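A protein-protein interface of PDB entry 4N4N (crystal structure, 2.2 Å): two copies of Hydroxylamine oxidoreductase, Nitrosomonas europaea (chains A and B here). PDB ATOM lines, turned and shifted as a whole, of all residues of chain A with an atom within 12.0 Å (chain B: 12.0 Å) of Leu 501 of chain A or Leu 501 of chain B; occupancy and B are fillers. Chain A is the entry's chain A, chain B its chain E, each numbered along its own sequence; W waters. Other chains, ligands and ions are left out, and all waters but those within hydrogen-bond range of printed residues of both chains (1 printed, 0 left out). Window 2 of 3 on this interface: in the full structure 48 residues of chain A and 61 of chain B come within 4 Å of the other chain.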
ATOM      1  N   LEU A 491       1.457  13.254  26.225  1.00  0.00           N
ATOM      2  CA  LEU A 491       1.657  14.693  26.097  1.00  0.00           C
ATOM      3  C   LEU A 491       3.147  15.052  26.134  1.00  0.00           C
ATOM      4  O   LEU A 491       3.597  15.921  25.381  1.00  0.00           O
ATOM      5  CB  LEU A 491       0.875  15.461  27.167  1.00  0.00           C
ATOM      6  CG  LEU A 491       0.904  16.994  27.124  1.00  0.00           C
ATOM      7  CD1 LEU A 491       0.475  17.539  25.763  1.00  0.00           C
ATOM      8  CD2 LEU A 491       0.033  17.573  28.234  1.00  0.00           C
ATOM      9  N   SER A 492       3.907  14.380  26.995  1.00  0.00           N
ATOM     10  CA  SER A 492       5.355  14.582  27.042  1.00  0.00           C
ATOM     11  C   SER A 492       6.034  13.970  25.813  1.00  0.00           C
ATOM     12  O   SER A 492       7.062  14.472  25.354  1.00  0.00           O
ATOM     13  CB  SER A 492       5.960  14.037  28.342  1.00  0.00           C
ATOM     14  OG  SER A 492       5.988  12.625  28.351  1.00  0.00           O
ATOM     15  N   ALA A 493       5.445  12.896  25.282  1.00  0.00           N
ATOM     16  CA  ALA A 493       5.896  12.300  24.021  1.00  0.00           C
ATOM     17  C   ALA A 493       5.713  13.275  22.857  1.00  0.00           C
ATOM     18  O   ALA A 493       6.601  13.417  22.018  1.00  0.00           O
ATOM     19  CB  ALA A 493       5.162  10.992  23.746  1.00  0.00           C
ATOM     20  N   LEU A 494       4.562  13.947  22.823  1.00  0.00           N
ATOM     21  CA  LEU A 494       4.273  14.960  21.809  1.00  0.00           C
ATOM     22  C   LEU A 494       5.215  16.163  21.934  1.00  0.00           C
ATOM     23  O   LEU A 494       5.685  16.695  20.927  1.00  0.00           O
ATOM     24  CB  LEU A 494       2.808  15.410  21.900  1.00  0.00           C
ATOM     25  CG  LEU A 494       2.263  16.385  20.845  1.00  0.00           C
ATOM     26  CD1 LEU A 494       2.132  15.724  19.478  1.00  0.00           C
ATOM     27  CD2 LEU A 494       0.926  16.962  21.285  1.00  0.00           C
ATOM     28  N   GLN A 495       5.484  16.573  23.172  1.00  0.00           N
ATOM     29  CA  GLN A 495       6.394  17.678  23.461  1.00  0.00           C
ATOM     30  C   GLN A 495       7.826  17.358  23.019  1.00  0.00           C
ATOM     31  O   GLN A 495       8.534  18.231  22.508  1.00  0.00           O
ATOM     32  CB  GLN A 495       6.354  18.018  24.956  1.00  0.00           C
ATOM     33  CG  GLN A 495       7.169  19.245  25.349  1.00  0.00           C
ATOM     34  CD  GLN A 495       6.944  19.676  26.787  1.00  0.00           C
ATOM     35  OE1 GLN A 495       7.897  19.942  27.521  1.00  0.00           O
ATOM     36  NE2 GLN A 495       5.678  19.750  27.197  1.00  0.00           N
ATOM     37  N   ALA A 496       8.235  16.106  23.221  1.00  0.00           N
ATOM     38  CA  ALA A 496       9.545  15.622  22.789  1.00  0.00           C
ATOM     39  C   ALA A 496       9.689  15.677  21.269  1.00  0.00           C
ATOM     40  O   ALA A 496      10.760  16.000  20.756  1.00  0.00           O
ATOM     41  CB  ALA A 496       9.784  14.208  23.301  1.00  0.00           C
ATOM     42  N   ARG A 497       8.602  15.365  20.561  1.00  0.00           N
ATOM     43  CA  ARG A 497       8.563  15.445  19.099  1.00  0.00           C
ATOM     44  C   ARG A 497       8.647  16.891  18.603  1.00  0.00           C
ATOM     45  O   ARG A 497       9.221  17.154  17.543  1.00  0.00           O
ATOM     46  CB  ARG A 497       7.308  14.765  18.543  1.00  0.00           C
ATOM     47  CG  ARG A 497       7.292  13.250  18.713  1.00  0.00           C
ATOM     48  CD  ARG A 497       6.393  12.575  17.683  1.00  0.00           C
ATOM     49  NE  ARG A 497       4.973  12.789  17.946  1.00  0.00           N
ATOM     50  CZ  ARG A 497       4.003  12.633  17.047  1.00  0.00           C
ATOM     51  NH1 ARG A 497       4.284  12.269  15.802  1.00  0.00           N
ATOM     52  NH2 ARG A 497       2.744  12.851  17.395  1.00  0.00           N
ATOM     53  N   VAL A 498       8.074  17.814  19.373  1.00  0.00           N
ATOM     54  CA  VAL A 498       8.158  19.247  19.082  1.00  0.00           C
ATOM     55  C   VAL A 498       9.588  19.747  19.311  1.00  0.00           C
ATOM     56  O   VAL A 498      10.106  20.542  18.523  1.00  0.00           O
ATOM     57  CB  VAL A 498       7.134  20.068  19.918  1.00  0.00           C
ATOM     58  CG1 VAL A 498       7.319  21.568  19.705  1.00  0.00           C
ATOM     59  CG2 VAL A 498       5.708  19.667  19.564  1.00  0.00           C
ATOM     60  N   ASN A 499      10.216  19.262  20.383  1.00  0.00           N
ATOM     61  CA  ASN A 499      11.624  19.543  20.669  1.00  0.00           C
ATOM     62  C   ASN A 499      12.542  19.138  19.514  1.00  0.00           C
ATOM     63  O   ASN A 499      13.506  19.842  19.206  1.00  0.00           O
ATOM     64  CB  ASN A 499      12.073  18.838  21.956  1.00  0.00           C
ATOM     65  CG  ASN A 499      11.448  19.434  23.210  1.00  0.00           C
ATOM     66  OD1 ASN A 499      10.926  20.551  23.200  1.00  0.00           O
ATOM     67  ND2 ASN A 499      11.510  18.684  24.307  1.00  0.00           N
ATOM     68  N   LYS A 500      12.233  18.003  18.885  1.00  0.00           N
ATOM     69  CA  LYS A 500      12.987  17.507  17.731  1.00  0.00           C
ATOM     70  C   LYS A 500      12.790  18.388  16.499  1.00  0.00           C
ATOM     71  O   LYS A 500      13.733  18.617  15.739  1.00  0.00           O
ATOM     72  CB  LYS A 500      12.604  16.059  17.404  1.00  0.00           C
ATOM     73  CG  LYS A 500      13.179  15.025  18.363  1.00  0.00           C
ATOM     74  CD  LYS A 500      12.721  13.618  17.992  1.00  0.00           C
ATOM     75  CE  LYS A 500      13.301  12.566  18.937  1.00  0.00           C
ATOM     76  NZ  LYS A 500      14.754  12.324  18.706  1.00  0.00           N
ATOM     77  N   LEU A 501      11.565  18.879  16.315  1.00  0.00           N
ATOM     78  CA  LEU A 501      11.241  19.786  15.211  1.00  0.00           C
ATOM     79  C   LEU A 501      11.851  21.178  15.395  1.00  0.00           C
ATOM     80  O   LEU A 501      11.914  21.965  14.446  1.00  0.00           O
ATOM     81  CB  LEU A 501       9.724  19.891  15.023  1.00  0.00           C
ATOM     82  CG  LEU A 501       8.994  18.701  14.391  1.00  0.00           C
ATOM     83  CD1 LEU A 501       7.499  18.792  14.657  1.00  0.00           C
ATOM     84  CD2 LEU A 501       9.273  18.601  12.892  1.00  0.00           C
ATOM     85  N   GLU A 502      12.295  21.472  16.616  1.00  0.00           N
ATOM     86  CA  GLU A 502      12.964  22.734  16.929  1.00  0.00           C
ATOM     87  C   GLU A 502      14.481  22.626  16.778  1.00  0.00           C
ATOM     88  O   GLU A 502      15.182  23.641  16.758  1.00  0.00           O
ATOM     89  CB  GLU A 502      12.603  23.201  18.341  1.00  0.00           C
ATOM     90  CG  GLU A 502      11.179  23.720  18.475  1.00  0.00           C
ATOM     91  CD  GLU A 502      10.820  24.122  19.898  1.00  0.00           C
ATOM     92  OE1 GLU A 502      11.488  23.666  20.852  1.00  0.00           O
ATOM     93  OE2 GLU A 502       9.857  24.898  20.057  1.00  0.00           O
ATOM     94  N   GLY A 503      14.977  21.392  16.674  1.00  0.00           N
ATOM     95  CA  GLY A 503      16.395  21.129  16.414  1.00  0.00           C
ATOM     96  C   GLY A 503      16.827  21.628  15.045  1.00  0.00           C
ATOM     97  O   GLY A 503      17.984  22.012  14.856  1.00  0.00           O
ATOM     98  N   LYS A 504      15.883  21.609  14.101  1.00  0.00           N
ATOM     99  CA  LYS A 504      16.029  22.170  12.745  1.00  0.00           C
ATOM    100  C   LYS A 504      17.352  21.857  12.041  1.00  0.00           C
ATOM    101  O   LYS A 504      17.509  22.110  10.844  1.00  0.00           O
ATOM    102  CB  LYS A 504      15.748  23.685  12.740  1.00  0.00           C
ATOM    103  CG  LYS A 504      16.920  24.571  13.160  1.00  0.00           C
ATOM    104  CD  LYS A 504      16.794  25.970  12.578  1.00  0.00           C
ATOM    105  CE  LYS A 504      18.102  26.741  12.700  1.00  0.00           C
ATOM    106  NZ  LYS A 504      18.049  28.052  11.992  1.00  0.00           N
ATOM    107  N   LEU B 491      -6.389  18.244  21.348  1.00  0.00           N
ATOM    108  CA  LEU B 491      -5.094  17.589  21.479  1.00  0.00           C
ATOM    109  C   LEU B 491      -4.830  16.663  20.290  1.00  0.00           C
ATOM    110  O   LEU B 491      -3.686  16.515  19.853  1.00  0.00           O
ATOM    111  CB  LEU B 491      -5.042  16.812  22.799  1.00  0.00           C
ATOM    112  CG  LEU B 491      -3.690  16.427  23.408  1.00  0.00           C
ATOM    113  CD1 LEU B 491      -3.766  16.481  24.931  1.00  0.00           C
ATOM    114  CD2 LEU B 491      -3.221  15.049  22.935  1.00  0.00           C
ATOM    115  N   SER B 492      -5.895  16.047  19.777  1.00  0.00           N
ATOM    116  CA  SER B 492      -5.822  15.192  18.591  1.00  0.00           C
ATOM    117  C   SER B 492      -5.444  15.998  17.347  1.00  0.00           C
ATOM    118  O   SER B 492      -4.647  15.543  16.527  1.00  0.00           O
ATOM    119  CB  SER B 492      -7.152  14.465  18.370  1.00  0.00           C
ATOM    120  OG  SER B 492      -7.075  13.577  17.270  1.00  0.00           O
ATOM    121  N   ALA B 493      -6.021  17.194  17.227  1.00  0.00           N
ATOM    122  CA  ALA B 493      -5.716  18.118  16.137  1.00  0.00           C
ATOM    123  C   ALA B 493      -4.300  18.684  16.242  1.00  0.00           C
ATOM    124  O   ALA B 493      -3.638  18.907  15.227  1.00  0.00           O
ATOM    125  CB  ALA B 493      -6.738  19.245  16.096  1.00  0.00           C
ATOM    126  N   LEU B 494      -3.839  18.911  17.471  1.00  0.00           N
ATOM    127  CA  LEU B 494      -2.469  19.358  17.711  1.00  0.00           C
ATOM    128  C   LEU B 494      -1.466  18.260  17.345  1.00  0.00           C
ATOM    129  O   LEU B 494      -0.392  18.547  16.809  1.00  0.00           O
ATOM    130  CB  LEU B 494      -2.286  19.806  19.167  1.00  0.00           C
ATOM    131  CG  LEU B 494      -0.990  20.527  19.566  1.00  0.00           C
ATOM    132  CD1 LEU B 494      -0.752  21.784  18.731  1.00  0.00           C
ATOM    133  CD2 LEU B 494      -1.006  20.870  21.053  1.00  0.00           C
ATOM    134  N   GLN B 495      -1.831  17.011  17.632  1.00  0.00           N
ATOM    135  CA  GLN B 495      -1.015  15.854  17.272  1.00  0.00           C
ATOM    136  C   GLN B 495      -0.955  15.689  15.753  1.00  0.00           C
ATOM    137  O   GLN B 495       0.085  15.321  15.204  1.00  0.00           O
ATOM    138  CB  GLN B 495      -1.566  14.585  17.927  1.00  0.00           C
ATOM    139  CG  GLN B 495      -0.632  13.380  17.863  1.00  0.00           C
ATOM    140  CD  GLN B 495      -1.206  12.149  18.546  1.00  0.00           C
ATOM    141  OE1 GLN B 495      -1.954  12.252  19.523  1.00  0.00           O
ATOM    142  NE2 GLN B 495      -0.849  10.973  18.040  1.00  0.00           N
ATOM    143  N   ALA B 496      -2.074  15.975  15.089  1.00  0.00           N
ATOM    144  CA  ALA B 496      -2.161  15.928  13.629  1.00  0.00           C
ATOM    145  C   ALA B 496      -1.267  16.982  12.975  1.00  0.00           C
ATOM    146  O   ALA B 496      -0.687  16.739  11.913  1.00  0.00           O
ATOM    147  CB  ALA B 496      -3.608  16.098  13.176  1.00  0.00           C
ATOM    148  N   ARG B 497      -1.159  18.144  13.614  1.00  0.00           N
ATOM    149  CA  ARG B 497      -0.313  19.229  13.113  1.00  0.00           C
ATOM    150  C   ARG B 497       1.179  18.928  13.254  1.00  0.00           C
ATOM    151  O   ARG B 497       1.981  19.344  12.415  1.00  0.00           O
ATOM    152  CB  ARG B 497      -0.669  20.559  13.784  1.00  0.00           C
ATOM    153  CG  ARG B 497      -2.007  21.134  13.333  1.00  0.00           C
ATOM    154  CD  ARG B 497      -2.068  22.636  13.546  1.00  0.00           C
ATOM    155  NE  ARG B 497      -2.425  23.001  14.913  1.00  0.00           N
ATOM    156  CZ  ARG B 497      -2.157  24.177  15.478  1.00  0.00           C
ATOM    157  NH1 ARG B 497      -1.501  25.119  14.809  1.00  0.00           N
ATOM    158  NH2 ARG B 497      -2.536  24.407  16.727  1.00  0.00           N
ATOM    159  N   VAL B 498       1.542  18.200  14.309  1.00  0.00           N
ATOM    160  CA  VAL B 498       2.921  17.749  14.518  1.00  0.00           C
ATOM    161  C   VAL B 498       3.274  16.638  13.520  1.00  0.00           C
ATOM    162  O   VAL B 498       4.405  16.573  13.030  1.00  0.00           O
ATOM    163  CB  VAL B 498       3.167  17.295  15.987  1.00  0.00           C
ATOM    164  CG1 VAL B 498       4.551  16.674  16.158  1.00  0.00           C
ATOM    165  CG2 VAL B 498       3.004  18.469  16.943  1.00  0.00           C
ATOM    166  N   ASN B 499       2.295  15.783  13.217  1.00  0.00           N
ATOM    167  CA  ASN B 499       2.434  14.756  12.181  1.00  0.00           C
ATOM    168  C   ASN B 499       2.734  15.347  10.801  1.00  0.00           C
ATOM    169  O   ASN B 499       3.578  14.827  10.068  1.00  0.00           O
ATOM    170  CB  ASN B 499       1.175  13.882  12.109  1.00  0.00           C
ATOM    171  CG  ASN B 499       1.077  12.884  13.252  1.00  0.00           C
ATOM    172  OD1 ASN B 499       2.080  12.514  13.867  1.00  0.00           O
ATOM    173  ND2 ASN B 499      -0.142  12.434  13.534  1.00  0.00           N
ATOM    174  N   LYS B 500       2.033  16.431  10.464  1.00  0.00           N
ATOM    175  CA  LYS B 500       2.224  17.153   9.205  1.00  0.00           C
ATOM    176  C   LYS B 500       3.641  17.704   9.064  1.00  0.00           C
ATOM    177  O   LYS B 500       4.270  17.556   8.014  1.00  0.00           O
ATOM    178  CB  LYS B 500       1.227  18.308   9.098  1.00  0.00           C
ATOM    179  CG  LYS B 500      -0.144  17.936   8.551  1.00  0.00           C
ATOM    180  CD  LYS B 500      -0.997  19.184   8.325  1.00  0.00           C
ATOM    181  CE  LYS B 500      -0.428  20.073   7.220  1.00  0.00           C
ATOM    182  NZ  LYS B 500      -0.961  21.463   7.284  1.00  0.00           N
ATOM    183  N   LEU B 501       4.130  18.337  10.129  1.00  0.00           N
ATOM    184  CA  LEU B 501       5.467  18.933  10.156  1.00  0.00           C
ATOM    185  C   LEU B 501       6.576  17.888  10.035  1.00  0.00           C
ATOM    186  O   LEU B 501       7.683  18.198   9.593  1.00  0.00           O
ATOM    187  CB  LEU B 501       5.663  19.756  11.435  1.00  0.00           C
ATOM    188  CG  LEU B 501       4.839  21.034  11.617  1.00  0.00           C
ATOM    189  CD1 LEU B 501       4.701  21.364  13.097  1.00  0.00           C
ATOM    190  CD2 LEU B 501       5.437  22.212  10.848  1.00  0.00           C
ATOM    191  N   GLU B 502       6.269  16.656  10.434  1.00  0.00           N
ATOM    192  CA  GLU B 502       7.221  15.550  10.359  1.00  0.00           C
ATOM    193  C   GLU B 502       7.235  14.888   8.981  1.00  0.00           C
ATOM    194  O   GLU B 502       8.291  14.459   8.508  1.00  0.00           O
ATOM    195  CB  GLU B 502       6.922  14.511  11.443  1.00  0.00           C
ATOM    196  CG  GLU B 502       7.338  14.948  12.843  1.00  0.00           C
ATOM    197  CD  GLU B 502       6.792  14.051  13.941  1.00  0.00           C
ATOM    198  OE1 GLU B 502       5.779  13.356  13.714  1.00  0.00           O
ATOM    199  OE2 GLU B 502       7.378  14.052  15.042  1.00  0.00           O
ATOM    200  N   GLY B 503       6.063  14.813   8.348  1.00  0.00           N
ATOM    201  CA  GLY B 503       5.910  14.166   7.042  1.00  0.00           C
ATOM    202  C   GLY B 503       6.651  14.866   5.916  1.00  0.00           C
ATOM    203  O   GLY B 503       6.927  16.065   5.988  1.00  0.00           O
HETATM  204  O   HOH W   1       9.871  14.398  15.960  1.00  0.00           O
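Water W1 bridges OE2 of Glu 502 of chain B and O of Arg 497 of chain A.
Of the printed residues of chain B, Leu 494 of chain A touches Gln 495 (3.8 Å) and Val 498 (3.8 Å). Printed residues of chain B within 4 Å of Arg 497 of chain A: Gln 495, Asn 499 and Glu 502. Val 498 of chain A touches just one residue of chain B: Val 498. No residue of chain B comes within 4 Å of Lys 500 of chain A. Leu 501 of chain A touches just these residues of chain B: Val 498 and Leu 501. No residue of chain B comes within 4 Å of Glu 502 of chain A. Gly 503 of chain A touches none of the printed residues of chain B. Lys 504 of chain A touches none of the printed residues of chain B. Of the printed residues of chain A, Gln 495 of chain B touches Leu 494 and Arg 497. Of the printed residues of chain A, Asn 499 of chain B touches Arg 497 (2.9 Å). No residue of chain A comes within 4 Å of Lys 500 of chain B. Leu 501 of chain B touches just one residue of chain A: Leu 501 (3.7 Å). No residue of chain A comes within 4 Å of Gly 503 of chain B. The nearest printed residue of chain A that does not touch Gln 495 of chain B is Leu 491 of chain A (7.6 Å).
NH1 of Arg 497 of chain A is in hydrogen-bond range of OD1 of Asn 499 of chain B (2.9 Å). NH1 of Arg 497 of chain A lies within salt-bridge range of OE1 of Glu 502 of chain B (2.8 Å).
Gln 495 of chain B touches Leu 494 of chain A. Leu 494 of chain A touches Val 498 of chain B. Arg 497 of chain A touches Gln 495 of chain B. Val 498 of chain A touches Val 498 of chain B (CG2 to CG2, 3.95 Å). Leu 501 of chain A touches Val 498 of chain B (CD1 to CG1, 3.9 Å). Leu 501 of chain B touches Leu 501 of chain A (O to CD2, 3.7 Å).
Arg 497 of chain A touches Glu 502 of chain B, but with the chains exchanged Glu 502 of chain A does not touch Arg 497 of chain B (11.3 Å). Val 498 of chain B touches its own counterpart, Val 498 of chain A. Leu 501 of chain A touches Val 498 of chain B, but with the chains exchanged Val 498 of chain A does not touch Leu 501 of chain B (6.8 Å). Leu 501 of chain B touches its own counterpart, Leu 501 of chain A. 13 positions are printed for both chains. Of the 8 pairs that touch across the chains among the printed residues, 2 have their exchanged pair printed and touching as well.
Of the 14 printed residues of chain A, 4 touch a printed residue of chain B. Hydrophobic or aromatic side chains of chain A that line the printed part of chain B: Leu 494, Val 498 and Leu 501. Among the printed residues, Asp or Glu carboxylates within 4 Å of a Lys or Arg side-chain nitrogen of the other chain: Arg 497 of chain A with Glu 502 of chain B (2.8 Å).
ND2 of Asn 499 of chain B sits close to O of Gln 495 of chain B, at 3.3 Å.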
